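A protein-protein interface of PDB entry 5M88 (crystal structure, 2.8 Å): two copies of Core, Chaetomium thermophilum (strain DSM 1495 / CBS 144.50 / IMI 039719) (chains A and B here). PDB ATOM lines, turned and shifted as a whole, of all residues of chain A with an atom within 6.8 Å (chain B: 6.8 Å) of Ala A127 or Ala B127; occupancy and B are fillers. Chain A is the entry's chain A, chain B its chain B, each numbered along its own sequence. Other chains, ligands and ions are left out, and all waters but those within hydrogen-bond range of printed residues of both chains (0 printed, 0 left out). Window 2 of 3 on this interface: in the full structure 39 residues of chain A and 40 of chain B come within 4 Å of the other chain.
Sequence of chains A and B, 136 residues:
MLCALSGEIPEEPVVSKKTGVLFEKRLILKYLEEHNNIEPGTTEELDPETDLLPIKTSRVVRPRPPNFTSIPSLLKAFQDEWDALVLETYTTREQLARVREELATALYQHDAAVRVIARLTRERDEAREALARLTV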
ATOM      1  N   ARG A 122     -28.269   1.803 -35.516  1.00  0.00           N
ATOM      2  CA  ARG A 122     -28.477   2.975 -34.671  1.00  0.00           C
ATOM      3  C   ARG A 122     -28.867   2.575 -33.253  1.00  0.00           C
ATOM      4  O   ARG A 122     -28.342   3.131 -32.280  1.00  0.00           O
ATOM      5  CB  ARG A 122     -29.533   3.894 -35.287  1.00  0.00           C
ATOM      6  CG  ARG A 122     -29.028   4.683 -36.488  1.00  0.00           C
ATOM      7  CD  ARG A 122     -27.743   5.433 -36.154  1.00  0.00           C
ATOM      8  NE  ARG A 122     -27.942   6.445 -35.120  1.00  0.00           N
ATOM      9  CZ  ARG A 122     -26.960   7.139 -34.552  1.00  0.00           C
ATOM     10  NH1 ARG A 122     -25.702   6.930 -34.916  1.00  0.00           N
ATOM     11  NH2 ARG A 122     -27.233   8.041 -33.619  1.00  0.00           N
ATOM     12  N   GLU A 123     -29.773   1.602 -33.112  1.00  0.00           N
ATOM     13  CA  GLU A 123     -30.195   1.184 -31.775  1.00  0.00           C
ATOM     14  C   GLU A 123     -29.053   0.520 -31.012  1.00  0.00           C
ATOM     15  O   GLU A 123     -28.862   0.778 -29.813  1.00  0.00           O
ATOM     16  CB  GLU A 123     -31.398   0.250 -31.884  1.00  0.00           C
ATOM     17  CG  GLU A 123     -32.666   0.949 -32.345  1.00  0.00           C
ATOM     18  CD  GLU A 123     -33.771  -0.021 -32.711  1.00  0.00           C
ATOM     19  OE1 GLU A 123     -33.467  -1.208 -32.948  1.00  0.00           O
ATOM     20  OE2 GLU A 123     -34.944   0.404 -32.759  1.00  0.00           O
ATOM     21  N   ARG A 124     -28.280  -0.333 -31.692  1.00  0.00           N
ATOM     22  CA  ARG A 124     -27.130  -0.979 -31.071  1.00  0.00           C
ATOM     23  C   ARG A 124     -26.113   0.048 -30.591  1.00  0.00           C
ATOM     24  O   ARG A 124     -25.586  -0.060 -29.477  1.00  0.00           O
ATOM     25  CB  ARG A 124     -26.499  -1.957 -32.066  1.00  0.00           C
ATOM     26  CG  ARG A 124     -25.374  -2.824 -31.518  1.00  0.00           C
ATOM     27  CD  ARG A 124     -24.009  -2.198 -31.755  1.00  0.00           C
ATOM     28  NE  ARG A 124     -23.790  -1.843 -33.153  1.00  0.00           N
ATOM     29  CZ  ARG A 124     -23.086  -2.575 -34.008  1.00  0.00           C
ATOM     30  NH1 ARG A 124     -22.522  -3.706 -33.607  1.00  0.00           N
ATOM     31  NH2 ARG A 124     -22.938  -2.175 -35.263  1.00  0.00           N
ATOM     32  N   ASP A 125     -25.827   1.061 -31.418  1.00  0.00           N
ATOM     33  CA  ASP A 125     -24.846   2.065 -31.027  1.00  0.00           C
ATOM     34  C   ASP A 125     -25.369   2.950 -29.903  1.00  0.00           C
ATOM     35  O   ASP A 125     -24.601   3.354 -29.023  1.00  0.00           O
ATOM     36  CB  ASP A 125     -24.439   2.903 -32.238  1.00  0.00           C
ATOM     37  CG  ASP A 125     -23.647   2.104 -33.254  1.00  0.00           C
ATOM     38  OD1 ASP A 125     -22.919   1.176 -32.837  1.00  0.00           O
ATOM     39  OD2 ASP A 125     -23.752   2.399 -34.464  1.00  0.00           O
ATOM     40  N   GLU A 126     -26.671   3.254 -29.902  1.00  0.00           N
ATOM     41  CA  GLU A 126     -27.242   4.000 -28.785  1.00  0.00           C
ATOM     42  C   GLU A 126     -27.095   3.226 -27.483  1.00  0.00           C
ATOM     43  O   GLU A 126     -26.704   3.792 -26.454  1.00  0.00           O
ATOM     44  CB  GLU A 126     -28.717   4.312 -29.043  1.00  0.00           C
ATOM     45  CG  GLU A 126     -28.968   5.410 -30.057  1.00  0.00           C
ATOM     46  CD  GLU A 126     -30.446   5.655 -30.281  1.00  0.00           C
ATOM     47  OE1 GLU A 126     -31.265   4.876 -29.746  1.00  0.00           O
ATOM     48  OE2 GLU A 126     -30.790   6.626 -30.988  1.00  0.00           O
ATOM     49  N   ALA A 127     -27.390   1.924 -27.512  1.00  0.00           N
ATOM     50  CA  ALA A 127     -27.265   1.126 -26.298  1.00  0.00           C
ATOM     51  C   ALA A 127     -25.810   1.013 -25.853  1.00  0.00           C
ATOM     52  O   ALA A 127     -25.514   1.108 -24.656  1.00  0.00           O
ATOM     53  CB  ALA A 127     -27.876  -0.257 -26.516  1.00  0.00           C
ATOM     54  N   ARG A 128     -24.884   0.834 -26.800  1.00  0.00           N
ATOM     55  CA  ARG A 128     -23.473   0.722 -26.434  1.00  0.00           C
ATOM     56  C   ARG A 128     -22.932   2.032 -25.876  1.00  0.00           C
ATOM     57  O   ARG A 128     -22.124   2.025 -24.940  1.00  0.00           O
ATOM     58  CB  ARG A 128     -22.646   0.273 -27.639  1.00  0.00           C
ATOM     59  CG  ARG A 128     -22.682  -1.221 -27.901  1.00  0.00           C
ATOM     60  CD  ARG A 128     -21.766  -1.594 -29.053  1.00  0.00           C
ATOM     61  NE  ARG A 128     -21.760  -3.031 -29.311  1.00  0.00           N
ATOM     62  CZ  ARG A 128     -21.176  -3.599 -30.363  1.00  0.00           C
ATOM     63  NH1 ARG A 128     -20.553  -2.851 -31.264  1.00  0.00           N
ATOM     64  NH2 ARG A 128     -21.221  -4.915 -30.519  1.00  0.00           N
ATOM     65  N   GLU A 129     -23.362   3.169 -26.431  1.00  0.00           N
ATOM     66  CA  GLU A 129     -22.923   4.455 -25.902  1.00  0.00           C
ATOM     67  C   GLU A 129     -23.525   4.722 -24.528  1.00  0.00           C
ATOM     68  O   GLU A 129     -22.857   5.285 -23.653  1.00  0.00           O
ATOM     69  CB  GLU A 129     -23.279   5.576 -26.879  1.00  0.00           C
ATOM     70  CG  GLU A 129     -22.697   6.928 -26.502  1.00  0.00           C
ATOM     71  CD  GLU A 129     -22.956   7.989 -27.554  1.00  0.00           C
ATOM     72  OE1 GLU A 129     -23.652   7.686 -28.547  1.00  0.00           O
ATOM     73  OE2 GLU A 129     -22.463   9.125 -27.387  1.00  0.00           O
ATOM     74  N   ALA A 130     -24.787   4.333 -24.320  1.00  0.00           N
ATOM     75  CA  ALA A 130     -25.378   4.436 -22.991  1.00  0.00           C
ATOM     76  C   ALA A 130     -24.653   3.548 -21.990  1.00  0.00           C
ATOM     77  O   ALA A 130     -24.560   3.890 -20.806  1.00  0.00           O
ATOM     78  CB  ALA A 130     -26.864   4.082 -23.043  1.00  0.00           C
ATOM     79  N   LEU A 131     -24.141   2.401 -22.446  1.00  0.00           N
ATOM     80  CA  LEU A 131     -23.382   1.525 -21.560  1.00  0.00           C
ATOM     81  C   LEU A 131     -22.002   2.100 -21.262  1.00  0.00           C
ATOM     82  O   LEU A 131     -21.479   1.930 -20.155  1.00  0.00           O
ATOM     83  CB  LEU A 131     -23.261   0.135 -22.186  1.00  0.00           C
ATOM     84  CG  LEU A 131     -22.818  -0.992 -21.258  1.00  0.00           C
ATOM     85  CD1 LEU A 131     -23.866  -1.237 -20.185  1.00  0.00           C
ATOM     86  CD2 LEU A 131     -22.563  -2.253 -22.058  1.00  0.00           C
ATOM     87  N   ALA A 132     -21.394   2.775 -22.241  1.00  0.00           N
ATOM     88  CA  ALA A 132     -20.107   3.424 -22.009  1.00  0.00           C
ATOM     89  C   ALA A 132     -20.235   4.560 -21.002  1.00  0.00           C
ATOM     90  O   ALA A 132     -19.251   4.923 -20.348  1.00  0.00           O
ATOM     91  CB  ALA A 132     -19.528   3.940 -23.325  1.00  0.00           C
ATOM     92  N   ARG B 122     -28.733  -9.634 -32.303  1.00  0.00           N
ATOM     93  CA  ARG B 122     -28.125 -10.240 -31.124  1.00  0.00           C
ATOM     94  C   ARG B 122     -27.302  -9.222 -30.346  1.00  0.00           C
ATOM     95  O   ARG B 122     -27.397  -9.149 -29.115  1.00  0.00           O
ATOM     96  CB  ARG B 122     -27.255 -11.431 -31.523  1.00  0.00           C
ATOM     97  CG  ARG B 122     -26.702 -12.201 -30.338  1.00  0.00           C
ATOM     98  CD  ARG B 122     -25.521 -13.070 -30.732  1.00  0.00           C
ATOM     99  NE  ARG B 122     -25.057 -13.885 -29.612  1.00  0.00           N
ATOM    100  CZ  ARG B 122     -23.931 -14.591 -29.617  1.00  0.00           C
ATOM    101  NH1 ARG B 122     -23.144 -14.587 -30.684  1.00  0.00           N
ATOM    102  NH2 ARG B 122     -23.592 -15.306 -28.552  1.00  0.00           N
ATOM    103  N   GLU B 123     -26.500  -8.416 -31.047  1.00  0.00           N
ATOM    104  CA  GLU B 123     -25.672  -7.427 -30.360  1.00  0.00           C
ATOM    105  C   GLU B 123     -26.525  -6.349 -29.700  1.00  0.00           C
ATOM    106  O   GLU B 123     -26.243  -5.926 -28.569  1.00  0.00           O
ATOM    107  CB  GLU B 123     -24.676  -6.804 -31.340  1.00  0.00           C
ATOM    108  CG  GLU B 123     -23.587  -7.763 -31.797  1.00  0.00           C
ATOM    109  CD  GLU B 123     -22.768  -7.216 -32.951  1.00  0.00           C
ATOM    110  OE1 GLU B 123     -23.237  -6.273 -33.624  1.00  0.00           O
ATOM    111  OE2 GLU B 123     -21.653  -7.727 -33.183  1.00  0.00           O
ATOM    112  N   ARG B 124     -27.570  -5.892 -30.394  1.00  0.00           N
ATOM    113  CA  ARG B 124     -28.486  -4.905 -29.836  1.00  0.00           C
ATOM    114  C   ARG B 124     -29.150  -5.430 -28.570  1.00  0.00           C
ATOM    115  O   ARG B 124     -29.247  -4.713 -27.565  1.00  0.00           O
ATOM    116  CB  ARG B 124     -29.526  -4.532 -30.899  1.00  0.00           C
ATOM    117  CG  ARG B 124     -30.480  -3.401 -30.543  1.00  0.00           C
ATOM    118  CD  ARG B 124     -31.764  -3.934 -29.933  1.00  0.00           C
ATOM    119  NE  ARG B 124     -32.386  -4.959 -30.764  1.00  0.00           N
ATOM    120  CZ  ARG B 124     -33.411  -4.741 -31.580  1.00  0.00           C
ATOM    121  NH1 ARG B 124     -33.938  -3.529 -31.672  1.00  0.00           N
ATOM    122  NH2 ARG B 124     -33.912  -5.736 -32.297  1.00  0.00           N
ATOM    123  N   ASP B 125     -29.595  -6.689 -28.591  1.00  0.00           N
ATOM    124  CA  ASP B 125     -30.260  -7.250 -27.421  1.00  0.00           C
ATOM    125  C   ASP B 125     -29.278  -7.474 -26.278  1.00  0.00           C
ATOM    126  O   ASP B 125     -29.624  -7.265 -25.110  1.00  0.00           O
ATOM    127  CB  ASP B 125     -30.965  -8.551 -27.797  1.00  0.00           C
ATOM    128  CG  ASP B 125     -32.134  -8.326 -28.736  1.00  0.00           C
ATOM    129  OD1 ASP B 125     -32.764  -7.252 -28.650  1.00  0.00           O
ATOM    130  OD2 ASP B 125     -32.421  -9.219 -29.561  1.00  0.00           O
ATOM    131  N   GLU B 126     -28.043  -7.873 -26.591  1.00  0.00           N
ATOM    132  CA  GLU B 126     -27.026  -8.010 -25.553  1.00  0.00           C
ATOM    133  C   GLU B 126     -26.746  -6.674 -24.877  1.00  0.00           C
ATOM    134  O   GLU B 126     -26.666  -6.595 -23.645  1.00  0.00           O
ATOM    135  CB  GLU B 126     -25.742  -8.590 -26.147  1.00  0.00           C
ATOM    136  CG  GLU B 126     -25.812 -10.077 -26.460  1.00  0.00           C
ATOM    137  CD  GLU B 126     -24.533 -10.608 -27.083  1.00  0.00           C
ATOM    138  OE1 GLU B 126     -23.641  -9.793 -27.400  1.00  0.00           O
ATOM    139  OE2 GLU B 126     -24.419 -11.840 -27.253  1.00  0.00           O
ATOM    140  N   ALA B 127     -26.609  -5.606 -25.669  1.00  0.00           N
ATOM    141  CA  ALA B 127     -26.342  -4.292 -25.091  1.00  0.00           C
ATOM    142  C   ALA B 127     -27.528  -3.788 -24.274  1.00  0.00           C
ATOM    143  O   ALA B 127     -27.346  -3.204 -23.198  1.00  0.00           O
ATOM    144  CB  ALA B 127     -25.981  -3.299 -26.195  1.00  0.00           C
ATOM    145  N   ARG B 128     -28.753  -4.007 -24.765  1.00  0.00           N
ATOM    146  CA  ARG B 128     -29.932  -3.563 -24.027  1.00  0.00           C
ATOM    147  C   ARG B 128     -30.096  -4.340 -22.725  1.00  0.00           C
ATOM    148  O   ARG B 128     -30.516  -3.774 -21.708  1.00  0.00           O
ATOM    149  CB  ARG B 128     -31.181  -3.690 -24.898  1.00  0.00           C
ATOM    150  CG  ARG B 128     -31.353  -2.543 -25.881  1.00  0.00           C
ATOM    151  CD  ARG B 128     -32.651  -2.655 -26.666  1.00  0.00           C
ATOM    152  NE  ARG B 128     -32.823  -1.531 -27.584  1.00  0.00           N
ATOM    153  CZ  ARG B 128     -33.781  -1.451 -28.502  1.00  0.00           C
ATOM    154  NH1 ARG B 128     -34.660  -2.436 -28.635  1.00  0.00           N
ATOM    155  NH2 ARG B 128     -33.855  -0.387 -29.292  1.00  0.00           N
ATOM    156  N   GLU B 129     -29.770  -5.634 -22.734  1.00  0.00           N
ATOM    157  CA  GLU B 129     -29.821  -6.411 -21.501  1.00  0.00           C
ATOM    158  C   GLU B 129     -28.736  -5.966 -20.531  1.00  0.00           C
ATOM    159  O   GLU B 129     -28.959  -5.928 -19.316  1.00  0.00           O
ATOM    160  CB  GLU B 129     -29.692  -7.902 -21.811  1.00  0.00           C
ATOM    161  CG  GLU B 129     -29.907  -8.802 -20.606  1.00  0.00           C
ATOM    162  CD  GLU B 129     -29.891 -10.275 -20.965  1.00  0.00           C
ATOM    163  OE1 GLU B 129     -29.642 -10.598 -22.146  1.00  0.00           O
ATOM    164  OE2 GLU B 129     -30.123 -11.109 -20.064  1.00  0.00           O
ATOM    165  N   ALA B 130     -27.552  -5.624 -21.048  1.00  0.00           N
ATOM    166  CA  ALA B 130     -26.506  -5.075 -20.192  1.00  0.00           C
ATOM    167  C   ALA B 130     -26.933  -3.754 -19.571  1.00  0.00           C
ATOM    168  O   ALA B 130     -26.566  -3.457 -18.428  1.00  0.00           O
ATOM    169  CB  ALA B 130     -25.212  -4.893 -20.986  1.00  0.00           C
ATOM    170  N   LEU B 131     -27.713  -2.952 -20.300  1.00  0.00           N
ATOM    171  CA  LEU B 131     -28.213  -1.706 -19.726  1.00  0.00           C
ATOM    172  C   LEU B 131     -29.319  -1.964 -18.708  1.00  0.00           C
ATOM    173  O   LEU B 131     -29.436  -1.224 -17.725  1.00  0.00           O
ATOM    174  CB  LEU B 131     -28.710  -0.774 -20.833  1.00  0.00           C
ATOM    175  CG  LEU B 131     -28.932   0.687 -20.431  1.00  0.00           C
ATOM    176  CD1 LEU B 131     -27.616   1.350 -20.047  1.00  0.00           C
ATOM    177  CD2 LEU B 131     -29.619   1.463 -21.545  1.00  0.00           C
ATOM    178  N   ALA B 132     -30.131  -3.004 -18.921  1.00  0.00           N
ATOM    179  CA  ALA B 132     -31.190  -3.329 -17.971  1.00  0.00           C
ATOM    180  C   ALA B 132     -30.634  -3.756 -16.617  1.00  0.00           C
ATOM    181  O   ALA B 132     -31.315  -3.610 -15.595  1.00  0.00           O
ATOM    182  CB  ALA B 132     -32.092  -4.425 -18.542  1.00  0.00           C
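OE2 of Glu B123 lies within salt-bridge range of NH2 of Arg A128, at 3.9 Å.
The side-chain carboxylate (OE1) of Glu A123 lies within salt-bridge range of the guanidinium group (NH1) of Arg B124, at 2.7 Å.
The side-chain carboxylate of Glu A123 lies within salt-bridge range of the guanidinium group of Arg B128 (3.7 Å).
The side-chain carboxylate (OE1) of Glu B123 lies within salt-bridge range of the guanidinium group (NH1) of Arg A124 (2.7 Å).
OD1 of Asp B125 lies within salt-bridge range of NE of Arg B124.
The guanidinium group (NE) of Arg A124 is in salt-bridge range of the side-chain carboxylate (OD1) of Asp A125 (3.2 Å).
Among the printed residues, pairs that only touch across the chains: Arg A124 with Arg B124, Ala A127 with Ala B127 and Leu A131 with Ala B130.
Of the printed residues of chain B, Ala A127 touches Ala B127.
Ala A130 touches none of the printed residues of chain B.
Of the printed residues of chain B, Leu A131 touches Ala B130.
Printed residues of chain A within 4 Å of Glu B123: Arg A124 (2.7 Å) and Arg A128 (3.7 Å).
Printed residues of chain A within 4 Å of Arg B124: Glu A123 and Arg A124.
Ala B127 touches one residue of chain A.
Of the printed residues of chain A, Arg B128 touches Glu A123 (3.4 Å).
Of the printed residues of chain A, Ala B130 touches Leu A131 (3.9 Å).
The nearest residue of chain A that does not touch Ala B127 is Arg A128 (4.3 Å).
The nearest printed residue of chain B that does not touch Leu A131 is Leu B131 (4.2 Å).
Of the 11 printed residues of chain A, 5 touch a printed residue of chain B.
Printed residues of chain A that touch a printed residue of chain B: Glu A123, Arg A124, Ala A127, Arg A128 and Leu A131.
Hydrophobic or aromatic side chains of chain A within 4 Å of the printed part of chain B: Ala A127 and Leu A131.
Printed residues of chain B that touch a printed residue of chain A: Glu B123, Arg B124, Ala B127, Arg B128 and Ala B130.
Hydrophobic or aromatic side chains of chain B that line the printed part of chain A: Ala B127 and Ala B130.
Among the printed residues, Asp or Glu carboxylates within 4 Å of a Lys or Arg side-chain nitrogen of the other chain: Glu A123 with Arg B124 (2.7 Å), Glu A123 with Arg B128 (3.7 Å), Arg A124 with Glu B123 (2.7 Å) and Arg A128 with Glu B123 (3.9 Å).
Glu A123 touches Arg B124, and with the chains exchanged Arg A124 touches Glu B123.
Glu A123 touches Arg B128, and with the chains exchanged Arg A128 touches Glu B123.
Arg A124 touches its own counterpart, Arg B124.
Leu A131 touches Ala B130, but with the chains exchanged Ala A130 does not touch Leu B131 (4.05 Å).
Positions printed for both chains: 122, 123, 124, 125, 126, 127, 128, 129, 130, 131 and 132.
Of the 7 pairs that touch across the chains among the printed residues, 6 have their exchanged pair printed and touching as well.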
